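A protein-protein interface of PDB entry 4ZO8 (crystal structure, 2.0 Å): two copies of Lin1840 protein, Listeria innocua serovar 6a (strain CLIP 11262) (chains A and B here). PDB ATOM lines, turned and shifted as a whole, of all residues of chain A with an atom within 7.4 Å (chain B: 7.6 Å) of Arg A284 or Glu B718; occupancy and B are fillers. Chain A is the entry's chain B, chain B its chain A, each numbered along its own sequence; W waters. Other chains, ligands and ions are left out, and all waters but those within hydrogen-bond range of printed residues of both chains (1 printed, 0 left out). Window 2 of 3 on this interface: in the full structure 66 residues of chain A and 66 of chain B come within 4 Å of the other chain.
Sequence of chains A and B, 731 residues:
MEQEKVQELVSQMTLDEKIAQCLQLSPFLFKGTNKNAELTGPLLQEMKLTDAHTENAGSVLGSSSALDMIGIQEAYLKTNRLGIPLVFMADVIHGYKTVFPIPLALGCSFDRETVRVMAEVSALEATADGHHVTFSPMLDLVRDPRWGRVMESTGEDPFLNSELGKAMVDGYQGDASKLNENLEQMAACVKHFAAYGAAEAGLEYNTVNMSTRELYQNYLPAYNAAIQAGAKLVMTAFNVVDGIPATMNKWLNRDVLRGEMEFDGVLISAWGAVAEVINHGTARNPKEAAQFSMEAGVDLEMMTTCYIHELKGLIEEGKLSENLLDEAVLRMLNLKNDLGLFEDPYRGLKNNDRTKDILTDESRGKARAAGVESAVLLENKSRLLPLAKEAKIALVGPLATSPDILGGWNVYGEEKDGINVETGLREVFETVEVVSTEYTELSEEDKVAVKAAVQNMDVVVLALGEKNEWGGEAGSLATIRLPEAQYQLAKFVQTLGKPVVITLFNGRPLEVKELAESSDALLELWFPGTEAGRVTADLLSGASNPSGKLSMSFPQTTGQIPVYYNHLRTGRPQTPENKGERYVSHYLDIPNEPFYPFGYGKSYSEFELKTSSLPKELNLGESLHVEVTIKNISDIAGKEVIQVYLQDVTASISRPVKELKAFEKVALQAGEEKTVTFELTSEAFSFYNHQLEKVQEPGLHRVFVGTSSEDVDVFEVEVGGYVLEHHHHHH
No position is printed for both chains.
Of the 7 pairs that touch across the chains among the printed residues, none has its exchanged pair printed and touching as well.
Of the 12 printed residues of chain A, 4 touch a printed residue of chain B.
Printed residues of chain A that touch a printed residue of chain B: Gly A281, Thr A282, Ala A283 and Arg A284.
Printed residues of chain B that touch a printed residue of chain A: Val B649, Thr B650, Ala B651 and Glu B718.
Along chain B the printed residues that touch a printed residue of chain A span positions 649 to 718.
Among the printed residues, 7 pairs touch across the chains.
Among the printed residues, Asp or Glu carboxylates within 4 Å of a Lys or Arg side-chain nitrogen of the other chain: Arg A284 with Glu B718.
Gly A281 touches Val B649 (CA to O, 3.5 Å).
Gly A281 touches Thr B650 (O to CA, 3.2 Å).
O of Ala B651 touches CA of Thr A282 (3.2 Å).
Ala A283 touches Thr B650.
Thr B650 touches Arg A284.
O of Gly A281 lies within hydrogen-bond range of N of Ala B651 (2.7 Å).
OE2 of Glu B718 lies within salt-bridge range of NH1 of Arg A284 (2.9 Å).
The backbone NH (N) of Thr A282 sits at hydrogen-bond distance from the backbone carbonyl oxygen (O) of Val A277 (3.0 Å).
N of Arg A284 lies within hydrogen-bond range of OE1 of Glu A288, at 2.9 Å.
The backbone carbonyl oxygen (O) of Lys B616 lies within hydrogen-bond range of the backbone NH (N) of Glu B718 (2.9 Å).
The backbone NH (N) of Val B649 is in hydrogen-bond range of the backbone carbonyl oxygen (O) of Leu B700 (3.2 Å).
The backbone carbonyl oxygen of Val A277 lies within hydrogen-bond range of the backbone NH of Ala A283 (3.5 Å).
The backbone carbonyl oxygen (O) of Glu B718 lies within hydrogen-bond range of the backbone NH (N) of Leu B618.
Of the printed residues of chain B, Gly A281 touches Val B649 (3.5 Å), Thr B650 (3.2 Å) and Ala B651 (2.7 Å).
Of the printed residues of chain B, Thr A282 touches Ala B651.
Ala A283 touches one residue of chain B.
Arg A284 touches just these residues of chain B: Thr B650 (3.5 Å) and Glu B718 (2.9 Å).
Glu A288 touches none of the printed residues of chain B.
Printed residues of chain A within 4 Å of Thr B650: Gly A281, Ala A283 and Arg A284.
Printed residues of chain A within 4 Å of Ala B651: Gly A281 (2.7 Å) and Thr A282 (3.2 Å).
Gly B699 touches none of the printed residues of chain A.
The nearest residue of chain B that does not touch Arg A284 is Leu B700 (4.1 Å).
The nearest printed residue of chain A that does not touch Thr B650 is Thr A282 (4.2 Å).
Water W1 lies within hydrogen-bond range of O of Ala A283 (2.7 Å), OG1 of Thr B650 (2.8 Å) and O of Ile A278 (3.2 Å).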
ATOM      1  N   VAL A 277       7.270  18.456  -2.760  1.00  0.00           N
ATOM      2  CA  VAL A 277       8.145  17.465  -3.341  1.00  0.00           C
ATOM      3  C   VAL A 277       7.604  17.023  -4.715  1.00  0.00           C
ATOM      4  O   VAL A 277       8.386  16.490  -5.533  1.00  0.00           O
ATOM      5  CB  VAL A 277       8.427  16.250  -2.413  1.00  0.00           C
ATOM      6  CG1 VAL A 277       8.927  16.701  -1.030  1.00  0.00           C
ATOM      7  CG2 VAL A 277       7.202  15.366  -2.304  1.00  0.00           C
ATOM      8  N   ILE A 278       6.288  17.240  -4.914  1.00  0.00           N
ATOM      9  CA  ILE A 278       5.641  17.028  -6.165  1.00  0.00           C
ATOM     10  C   ILE A 278       6.159  18.034  -7.188  1.00  0.00           C
ATOM     11  O   ILE A 278       6.590  17.642  -8.256  1.00  0.00           O
ATOM     12  CB  ILE A 278       4.108  17.137  -6.029  1.00  0.00           C
ATOM     13  CG1 ILE A 278       3.564  15.991  -5.225  1.00  0.00           C
ATOM     14  CG2 ILE A 278       3.455  17.186  -7.388  1.00  0.00           C
ATOM     15  CD1 ILE A 278       2.294  16.346  -4.489  1.00  0.00           C
ATOM     16  N   GLY A 281       9.351  17.302  -8.448  1.00  0.00           N
ATOM     17  CA  GLY A 281       9.393  16.144  -9.365  1.00  0.00           C
ATOM     18  C   GLY A 281       9.935  14.854  -8.762  1.00  0.00           C
ATOM     19  O   GLY A 281      10.433  14.013  -9.454  1.00  0.00           O
ATOM     20  N   THR A 282       9.814  14.682  -7.452  1.00  0.00           N
ATOM     21  CA  THR A 282      10.215  13.453  -6.811  1.00  0.00           C
ATOM     22  C   THR A 282       9.063  12.708  -6.134  1.00  0.00           C
ATOM     23  O   THR A 282       9.264  11.751  -5.378  1.00  0.00           O
ATOM     24  CB  THR A 282      11.398  13.692  -5.801  1.00  0.00           C
ATOM     25  OG1 THR A 282      11.015  14.640  -4.826  1.00  0.00           O
ATOM     26  CG2 THR A 282      12.637  14.196  -6.504  1.00  0.00           C
ATOM     27  N   ALA A 283       7.857  13.183  -6.385  1.00  0.00           N
ATOM     28  CA  ALA A 283       6.615  12.450  -6.087  1.00  0.00           C
ATOM     29  C   ALA A 283       5.633  12.794  -7.188  1.00  0.00           C
ATOM     30  O   ALA A 283       5.618  13.942  -7.631  1.00  0.00           O
ATOM     31  CB  ALA A 283       6.043  12.838  -4.741  1.00  0.00           C
ATOM     32  N   ARG A 284       4.854  11.812  -7.635  1.00  0.00           N
ATOM     33  CA  ARG A 284       3.864  12.001  -8.718  1.00  0.00           C
ATOM     34  C   ARG A 284       2.642  12.767  -8.224  1.00  0.00           C
ATOM     35  O   ARG A 284       2.021  13.492  -8.951  1.00  0.00           O
ATOM     36  CB  ARG A 284       3.486  10.624  -9.387  1.00  0.00           C
ATOM     37  CG  ARG A 284       2.831  10.687 -10.770  1.00  0.00           C
ATOM     38  CD  ARG A 284       2.839   9.346 -11.549  1.00  0.00           C
ATOM     39  NE  ARG A 284       2.379   9.556 -12.924  1.00  0.00           N
ATOM     40  CZ  ARG A 284       2.553   8.723 -13.974  1.00  0.00           C
ATOM     41  NH1 ARG A 284       2.042   9.036 -15.169  1.00  0.00           N
ATOM     42  NH2 ARG A 284       3.231   7.580 -13.863  1.00  0.00           N
ATOM     43  N   ASN A 285       2.317  12.631  -6.966  1.00  0.00           N
ATOM     44  CA  ASN A 285       0.994  13.013  -6.478  1.00  0.00           C
ATOM     45  C   ASN A 285       0.996  13.072  -4.967  1.00  0.00           C
ATOM     46  O   ASN A 285       2.015  12.760  -4.354  1.00  0.00           O
ATOM     47  CB  ASN A 285      -0.092  12.059  -6.968  1.00  0.00           C
ATOM     48  CG  ASN A 285       0.176  10.613  -6.625  1.00  0.00           C
ATOM     49  OD1 ASN A 285       0.867  10.289  -5.684  1.00  0.00           O
ATOM     50  ND2 ASN A 285      -0.409   9.736  -7.371  1.00  0.00           N
ATOM     51  N   PRO A 286      -0.116  13.523  -4.352  1.00  0.00           N
ATOM     52  CA  PRO A 286      -0.030  13.593  -2.864  1.00  0.00           C
ATOM     53  C   PRO A 286       0.074  12.235  -2.144  1.00  0.00           C
ATOM     54  O   PRO A 286       0.570  12.152  -1.005  1.00  0.00           O
ATOM     55  CB  PRO A 286      -1.309  14.322  -2.466  1.00  0.00           C
ATOM     56  CG  PRO A 286      -1.686  15.123  -3.699  1.00  0.00           C
ATOM     57  CD  PRO A 286      -1.161  14.398  -4.922  1.00  0.00           C
ATOM     58  N   LYS A 287      -0.396  11.171  -2.775  1.00  0.00           N
ATOM     59  CA  LYS A 287      -0.225   9.836  -2.186  1.00  0.00           C
ATOM     60  C   LYS A 287       1.281   9.505  -2.103  1.00  0.00           C
ATOM     61  O   LYS A 287       1.766   9.001  -1.093  1.00  0.00           O
ATOM     62  CB  LYS A 287      -0.990   8.783  -3.006  1.00  0.00           C
ATOM     63  CG  LYS A 287      -0.905   7.394  -2.446  1.00  0.00           C
ATOM     64  CD  LYS A 287      -1.641   6.412  -3.343  1.00  0.00           C
ATOM     65  CE  LYS A 287      -2.259   5.273  -2.539  1.00  0.00           C
ATOM     66  NZ  LYS A 287      -2.869   4.273  -3.458  1.00  0.00           N
ATOM     67  N   GLU A 288       2.020   9.782  -3.161  1.00  0.00           N
ATOM     68  CA  GLU A 288       3.470   9.494  -3.138  1.00  0.00           C
ATOM     69  C   GLU A 288       4.183  10.404  -2.124  1.00  0.00           C
ATOM     70  O   GLU A 288       4.961   9.918  -1.338  1.00  0.00           O
ATOM     71  CB  GLU A 288       4.105   9.565  -4.538  1.00  0.00           C
ATOM     72  CG  GLU A 288       3.915   8.277  -5.323  1.00  0.00           C
ATOM     73  CD  GLU A 288       4.629   8.241  -6.669  1.00  0.00           C
ATOM     74  OE1 GLU A 288       5.504   9.126  -6.919  1.00  0.00           O
ATOM     75  OE2 GLU A 288       4.292   7.325  -7.466  1.00  0.00           O
ATOM     76  N   ALA A 289       3.845  11.698  -2.108  1.00  0.00           N
ATOM     77  CA  ALA A 289       4.447  12.670  -1.196  1.00  0.00           C
ATOM     78  C   ALA A 289       4.326  12.247   0.238  1.00  0.00           C
ATOM     79  O   ALA A 289       5.331  12.286   1.011  1.00  0.00           O
ATOM     80  CB  ALA A 289       3.820  14.034  -1.398  1.00  0.00           C
ATOM     81  N   PHE A 292       6.453   8.997   0.962  1.00  0.00           N
ATOM     82  CA  PHE A 292       7.902   9.303   1.052  1.00  0.00           C
ATOM     83  C   PHE A 292       8.251  10.178   2.242  1.00  0.00           C
ATOM     84  O   PHE A 292       9.289  10.038   2.850  1.00  0.00           O
ATOM     85  CB  PHE A 292       8.445   9.894  -0.262  1.00  0.00           C
ATOM     86  CG  PHE A 292       8.133   9.056  -1.481  1.00  0.00           C
ATOM     87  CD1 PHE A 292       8.010   7.657  -1.401  1.00  0.00           C
ATOM     88  CD2 PHE A 292       8.059   9.646  -2.728  1.00  0.00           C
ATOM     89  CE1 PHE A 292       7.772   6.884  -2.539  1.00  0.00           C
ATOM     90  CE2 PHE A 292       7.794   8.880  -3.888  1.00  0.00           C
ATOM     91  CZ  PHE A 292       7.630   7.501  -3.784  1.00  0.00           C
ATOM     92  N   PRO B 615       4.264   7.705 -30.385  1.00  0.00           N
ATOM     93  CA  PRO B 615       3.500   6.788 -29.496  1.00  0.00           C
ATOM     94  C   PRO B 615       3.136   7.379 -28.109  1.00  0.00           C
ATOM     95  O   PRO B 615       3.781   8.291 -27.616  1.00  0.00           O
ATOM     96  CB  PRO B 615       4.450   5.584 -29.322  1.00  0.00           C
ATOM     97  CG  PRO B 615       5.823   6.115 -29.688  1.00  0.00           C
ATOM     98  CD  PRO B 615       5.566   7.146 -30.764  1.00  0.00           C
ATOM     99  N   LYS B 616       2.089   6.854 -27.493  1.00  0.00           N
ATOM    100  CA  LYS B 616       1.664   7.281 -26.144  1.00  0.00           C
ATOM    101  C   LYS B 616       2.474   6.533 -25.073  1.00  0.00           C
ATOM    102  O   LYS B 616       2.616   7.014 -23.942  1.00  0.00           O
ATOM    103  CB  LYS B 616       0.167   7.007 -25.926  1.00  0.00           C
ATOM    104  CG  LYS B 616      -0.617   8.066 -25.132  1.00  0.00           C
ATOM    105  CD  LYS B 616      -0.175   8.281 -23.679  1.00  0.00           C
ATOM    106  CE  LYS B 616       0.646   9.553 -23.469  1.00  0.00           C
ATOM    107  NZ  LYS B 616       0.503  10.036 -22.065  1.00  0.00           N
ATOM    108  N   GLU B 617       2.962   5.354 -25.427  1.00  0.00           N
ATOM    109  CA  GLU B 617       3.663   4.476 -24.523  1.00  0.00           C
ATOM    110  C   GLU B 617       4.903   3.929 -25.195  1.00  0.00           C
ATOM    111  O   GLU B 617       4.978   3.879 -26.401  1.00  0.00           O
ATOM    112  CB  GLU B 617       2.803   3.277 -24.143  1.00  0.00           C
ATOM    113  CG  GLU B 617       1.321   3.584 -23.984  1.00  0.00           C
ATOM    114  CD  GLU B 617       0.629   2.633 -23.026  1.00  0.00           C
ATOM    115  OE1 GLU B 617       0.790   2.833 -21.811  1.00  0.00           O
ATOM    116  OE2 GLU B 617      -0.079   1.697 -23.487  1.00  0.00           O
ATOM    117  N   LEU B 618       5.834   3.473 -24.366  1.00  0.00           N
ATOM    118  CA  LEU B 618       7.139   2.963 -24.769  1.00  0.00           C
ATOM    119  C   LEU B 618       7.520   1.941 -23.729  1.00  0.00           C
ATOM    120  O   LEU B 618       7.247   2.156 -22.538  1.00  0.00           O
ATOM    121  CB  LEU B 618       8.184   4.108 -24.712  1.00  0.00           C
ATOM    122  CG  LEU B 618       9.200   4.255 -25.818  1.00  0.00           C
ATOM    123  CD1 LEU B 618       8.522   4.286 -27.197  1.00  0.00           C
ATOM    124  CD2 LEU B 618       9.980   5.549 -25.616  1.00  0.00           C
ATOM    125  N   ASN B 619       8.151   0.837 -24.127  1.00  0.00           N
ATOM    126  CA  ASN B 619       8.768  -0.060 -23.126  1.00  0.00           C
ATOM    127  C   ASN B 619      10.079   0.509 -22.566  1.00  0.00           C
ATOM    128  O   ASN B 619      10.707   1.313 -23.198  1.00  0.00           O
ATOM    129  CB  ASN B 619       9.009  -1.444 -23.701  1.00  0.00           C
ATOM    130  CG  ASN B 619       7.712  -2.157 -24.060  1.00  0.00           C
ATOM    131  OD1 ASN B 619       7.525  -2.557 -25.189  1.00  0.00           O
ATOM    132  ND2 ASN B 619       6.843  -2.317 -23.109  1.00  0.00           N
ATOM    133  N   LEU B 620      10.470   0.087 -21.373  1.00  0.00           N
ATOM    134  CA  LEU B 620      11.785   0.363 -20.878  1.00  0.00           C
ATOM    135  C   LEU B 620      12.796  -0.213 -21.893  1.00  0.00           C
ATOM    136  O   LEU B 620      12.534  -1.248 -22.521  1.00  0.00           O
ATOM    137  CB  LEU B 620      11.969  -0.230 -19.493  1.00  0.00           C
ATOM    138  CG  LEU B 620      11.119   0.449 -18.427  1.00  0.00           C
ATOM    139  CD1 LEU B 620      10.789  -0.482 -17.260  1.00  0.00           C
ATOM    140  CD2 LEU B 620      11.816   1.752 -17.954  1.00  0.00           C
ATOM    141  N   VAL B 649       9.480  13.704 -15.763  1.00  0.00           N
ATOM    142  CA  VAL B 649       8.563  14.519 -14.948  1.00  0.00           C
ATOM    143  C   VAL B 649       8.658  14.207 -13.472  1.00  0.00           C
ATOM    144  O   VAL B 649       8.623  15.104 -12.641  1.00  0.00           O
ATOM    145  CB  VAL B 649       7.134  14.363 -15.448  1.00  0.00           C
ATOM    146  CG1 VAL B 649       6.125  14.953 -14.489  1.00  0.00           C
ATOM    147  CG2 VAL B 649       6.983  15.047 -16.801  1.00  0.00           C
ATOM    148  N   THR B 650       8.782  12.918 -13.149  1.00  0.00           N
ATOM    149  CA  THR B 650       8.846  12.454 -11.758  1.00  0.00           C
ATOM    150  C   THR B 650       9.920  11.445 -11.634  1.00  0.00           C
ATOM    151  O   THR B 650       9.986  10.523 -12.425  1.00  0.00           O
ATOM    152  CB  THR B 650       7.548  11.805 -11.328  1.00  0.00           C
ATOM    153  OG1 THR B 650       6.483  12.708 -11.673  1.00  0.00           O
ATOM    154  CG2 THR B 650       7.578  11.496  -9.854  1.00  0.00           C
ATOM    155  N   ALA B 651      10.849  11.644 -10.718  1.00  0.00           N
ATOM    156  CA  ALA B 651      11.938  10.697 -10.645  1.00  0.00           C
ATOM    157  C   ALA B 651      12.481  10.640  -9.225  1.00  0.00           C
ATOM    158  O   ALA B 651      12.060  11.391  -8.398  1.00  0.00           O
ATOM    159  CB  ALA B 651      13.026  11.070 -11.665  1.00  0.00           C
ATOM    160  N   PHE B 685      16.824   8.564 -21.913  1.00  0.00           N
ATOM    161  CA  PHE B 685      15.810   8.563 -20.840  1.00  0.00           C
ATOM    162  C   PHE B 685      16.351   8.255 -19.431  1.00  0.00           C
ATOM    163  O   PHE B 685      15.595   8.213 -18.448  1.00  0.00           O
ATOM    164  CB  PHE B 685      14.720   7.509 -21.164  1.00  0.00           C
ATOM    165  CG  PHE B 685      13.840   7.855 -22.329  1.00  0.00           C
ATOM    166  CD1 PHE B 685      14.254   7.646 -23.617  1.00  0.00           C
ATOM    167  CD2 PHE B 685      12.562   8.355 -22.122  1.00  0.00           C
ATOM    168  CE1 PHE B 685      13.430   7.956 -24.698  1.00  0.00           C
ATOM    169  CE2 PHE B 685      11.741   8.648 -23.197  1.00  0.00           C
ATOM    170  CZ  PHE B 685      12.184   8.459 -24.486  1.00  0.00           C
ATOM    171  N   PRO B 698      10.518   3.529 -15.012  1.00  0.00           N
ATOM    172  CA  PRO B 698       9.193   3.751 -15.604  1.00  0.00           C
ATOM    173  C   PRO B 698       8.523   5.059 -15.162  1.00  0.00           C
ATOM    174  O   PRO B 698       8.744   5.550 -14.027  1.00  0.00           O
ATOM    175  CB  PRO B 698       8.368   2.550 -15.136  1.00  0.00           C
ATOM    176  CG  PRO B 698       9.049   2.038 -13.917  1.00  0.00           C
ATOM    177  CD  PRO B 698      10.511   2.410 -14.044  1.00  0.00           C
ATOM    178  N   GLY B 699       7.706   5.604 -16.063  1.00  0.00           N
ATOM    179  CA  GLY B 699       6.992   6.824 -15.783  1.00  0.00           C
ATOM    180  C   GLY B 699       6.891   7.774 -16.972  1.00  0.00           C
ATOM    181  O   GLY B 699       7.253   7.406 -18.119  1.00  0.00           O
ATOM    182  N   LEU B 700       6.423   9.004 -16.673  1.00  0.00           N
ATOM    183  CA  LEU B 700       6.080   9.994 -17.705  1.00  0.00           C
ATOM    184  C   LEU B 700       7.283  10.796 -18.151  1.00  0.00           C
ATOM    185  O   LEU B 700       7.988  11.316 -17.320  1.00  0.00           O
ATOM    186  CB  LEU B 700       5.022  10.984 -17.184  1.00  0.00           C
ATOM    187  CG  LEU B 700       4.398  12.026 -18.151  1.00  0.00           C
ATOM    188  CD1 LEU B 700       3.556  11.422 -19.277  1.00  0.00           C
ATOM    189  CD2 LEU B 700       3.540  12.995 -17.359  1.00  0.00           C
ATOM    190  N   HIS B 701       7.452  10.956 -19.457  1.00  0.00           N
ATOM    191  CA  HIS B 701       8.399  11.905 -19.995  1.00  0.00           C
ATOM    192  C   HIS B 701       7.643  12.822 -20.923  1.00  0.00           C
ATOM    193  O   HIS B 701       6.552  12.459 -21.450  1.00  0.00           O
ATOM    194  CB  HIS B 701       9.492  11.183 -20.767  1.00  0.00           C
ATOM    195  CG  HIS B 701      10.392  10.341 -19.906  1.00  0.00           C
ATOM    196  ND1 HIS B 701      11.697  10.677 -19.627  1.00  0.00           N
ATOM    197  CD2 HIS B 701      10.148   9.203 -19.223  1.00  0.00           C
ATOM    198  CE1 HIS B 701      12.207   9.793 -18.786  1.00  0.00           C
ATOM    199  NE2 HIS B 701      11.303   8.859 -18.567  1.00  0.00           N
ATOM    200  N   ARG B 702       8.135  14.043 -21.032  1.00  0.00           N
ATOM    201  CA  ARG B 702       7.700  15.001 -22.035  1.00  0.00           C
ATOM    202  C   ARG B 702       8.840  15.156 -23.010  1.00  0.00           C
ATOM    203  O   ARG B 702       9.986  15.141 -22.611  1.00  0.00           O
ATOM    204  CB  ARG B 702       7.371  16.377 -21.445  1.00  0.00           C
ATOM    205  CG  ARG B 702       6.186  16.400 -20.487  1.00  0.00           C
ATOM    206  CD  ARG B 702       5.939  17.815 -20.030  1.00  0.00           C
ATOM    207  NE  ARG B 702       4.886  17.740 -19.052  1.00  0.00           N
ATOM    208  CZ  ARG B 702       5.005  17.953 -17.733  1.00  0.00           C
ATOM    209  NH1 ARG B 702       6.142  18.377 -17.188  1.00  0.00           N
ATOM    210  NH2 ARG B 702       3.945  17.774 -16.961  1.00  0.00           N
ATOM    211  N   GLU B 716       3.699  14.009 -24.704  1.00  0.00           N
ATOM    212  CA  GLU B 716       3.820  13.136 -23.530  1.00  0.00           C
ATOM    213  C   GLU B 716       3.959  11.693 -23.912  1.00  0.00           C
ATOM    214  O   GLU B 716       3.320  11.245 -24.838  1.00  0.00           O
ATOM    215  CB  GLU B 716       2.687  13.361 -22.502  1.00  0.00           C
ATOM    216  CG  GLU B 716       2.960  14.679 -21.758  1.00  0.00           C
ATOM    217  CD  GLU B 716       1.928  15.120 -20.750  1.00  0.00           C
ATOM    218  OE1 GLU B 716       1.048  14.305 -20.401  1.00  0.00           O
ATOM    219  OE2 GLU B 716       2.058  16.298 -20.304  1.00  0.00           O
ATOM    220  N   VAL B 717       4.889  11.004 -23.232  1.00  0.00           N
ATOM    221  CA  VAL B 717       5.159   9.562 -23.428  1.00  0.00           C
ATOM    222  C   VAL B 717       5.310   8.864 -22.117  1.00  0.00           C
ATOM    223  O   VAL B 717       6.212   9.206 -21.345  1.00  0.00           O
ATOM    224  CB  VAL B 717       6.461   9.247 -24.191  1.00  0.00           C
ATOM    225  CG1 VAL B 717       6.488   7.772 -24.495  1.00  0.00           C
ATOM    226  CG2 VAL B 717       6.485  10.020 -25.469  1.00  0.00           C
ATOM    227  N   GLU B 718       4.452   7.876 -21.894  1.00  0.00           N
ATOM    228  CA  GLU B 718       4.462   7.079 -20.685  1.00  0.00           C
ATOM    229  C   GLU B 718       5.348   5.840 -20.897  1.00  0.00           C
ATOM    230  O   GLU B 718       4.974   4.930 -21.636  1.00  0.00           O
ATOM    231  CB  GLU B 718       3.036   6.681 -20.329  1.00  0.00           C
ATOM    232  CG  GLU B 718       2.869   6.107 -18.928  1.00  0.00           C
ATOM    233  CD  GLU B 718       3.233   7.070 -17.818  1.00  0.00           C
ATOM    234  OE1 GLU B 718       3.860   6.616 -16.847  1.00  0.00           O
ATOM    235  OE2 GLU B 718       2.878   8.257 -17.864  1.00  0.00           O
ATOM    236  N   VAL B 719       6.536   5.847 -20.286  1.00  0.00           N
ATOM    237  CA  VAL B 719       7.437   4.680 -20.256  1.00  0.00           C
ATOM    238  C   VAL B 719       7.145   3.673 -19.131  1.00  0.00           C
ATOM    239  O   VAL B 719       7.057   4.047 -17.963  1.00  0.00           O
ATOM    240  CB  VAL B 719       8.923   5.100 -20.201  1.00  0.00           C
ATOM    241  CG1 VAL B 719       9.818   3.906 -20.426  1.00  0.00           C
ATOM    242  CG2 VAL B 719       9.241   6.138 -21.271  1.00  0.00           C
ATOM    243  N   GLY B 720       6.960   2.399 -19.495  1.00  0.00           N
ATOM    244  CA  GLY B 720       6.917   1.310 -18.511  1.00  0.00           C
ATOM    245  C   GLY B 720       6.915  -0.084 -19.076  1.00  0.00           C
ATOM    246  O   GLY B 720       7.276  -0.274 -20.200  1.00  0.00           O
ATOM    247  N   GLY B 721       6.505  -1.066 -18.273  1.00  0.00           N
ATOM    248  CA  GLY B 721       6.262  -2.446 -18.742  1.00  0.00           C
ATOM    249  C   GLY B 721       7.516  -3.302 -18.657  1.00  0.00           C
ATOM    250  O   GLY B 721       8.226  -3.278 -17.621  1.00  0.00           O
HETATM  251  O   HOH W   1       6.092  15.031 -10.073  1.00  0.00           O
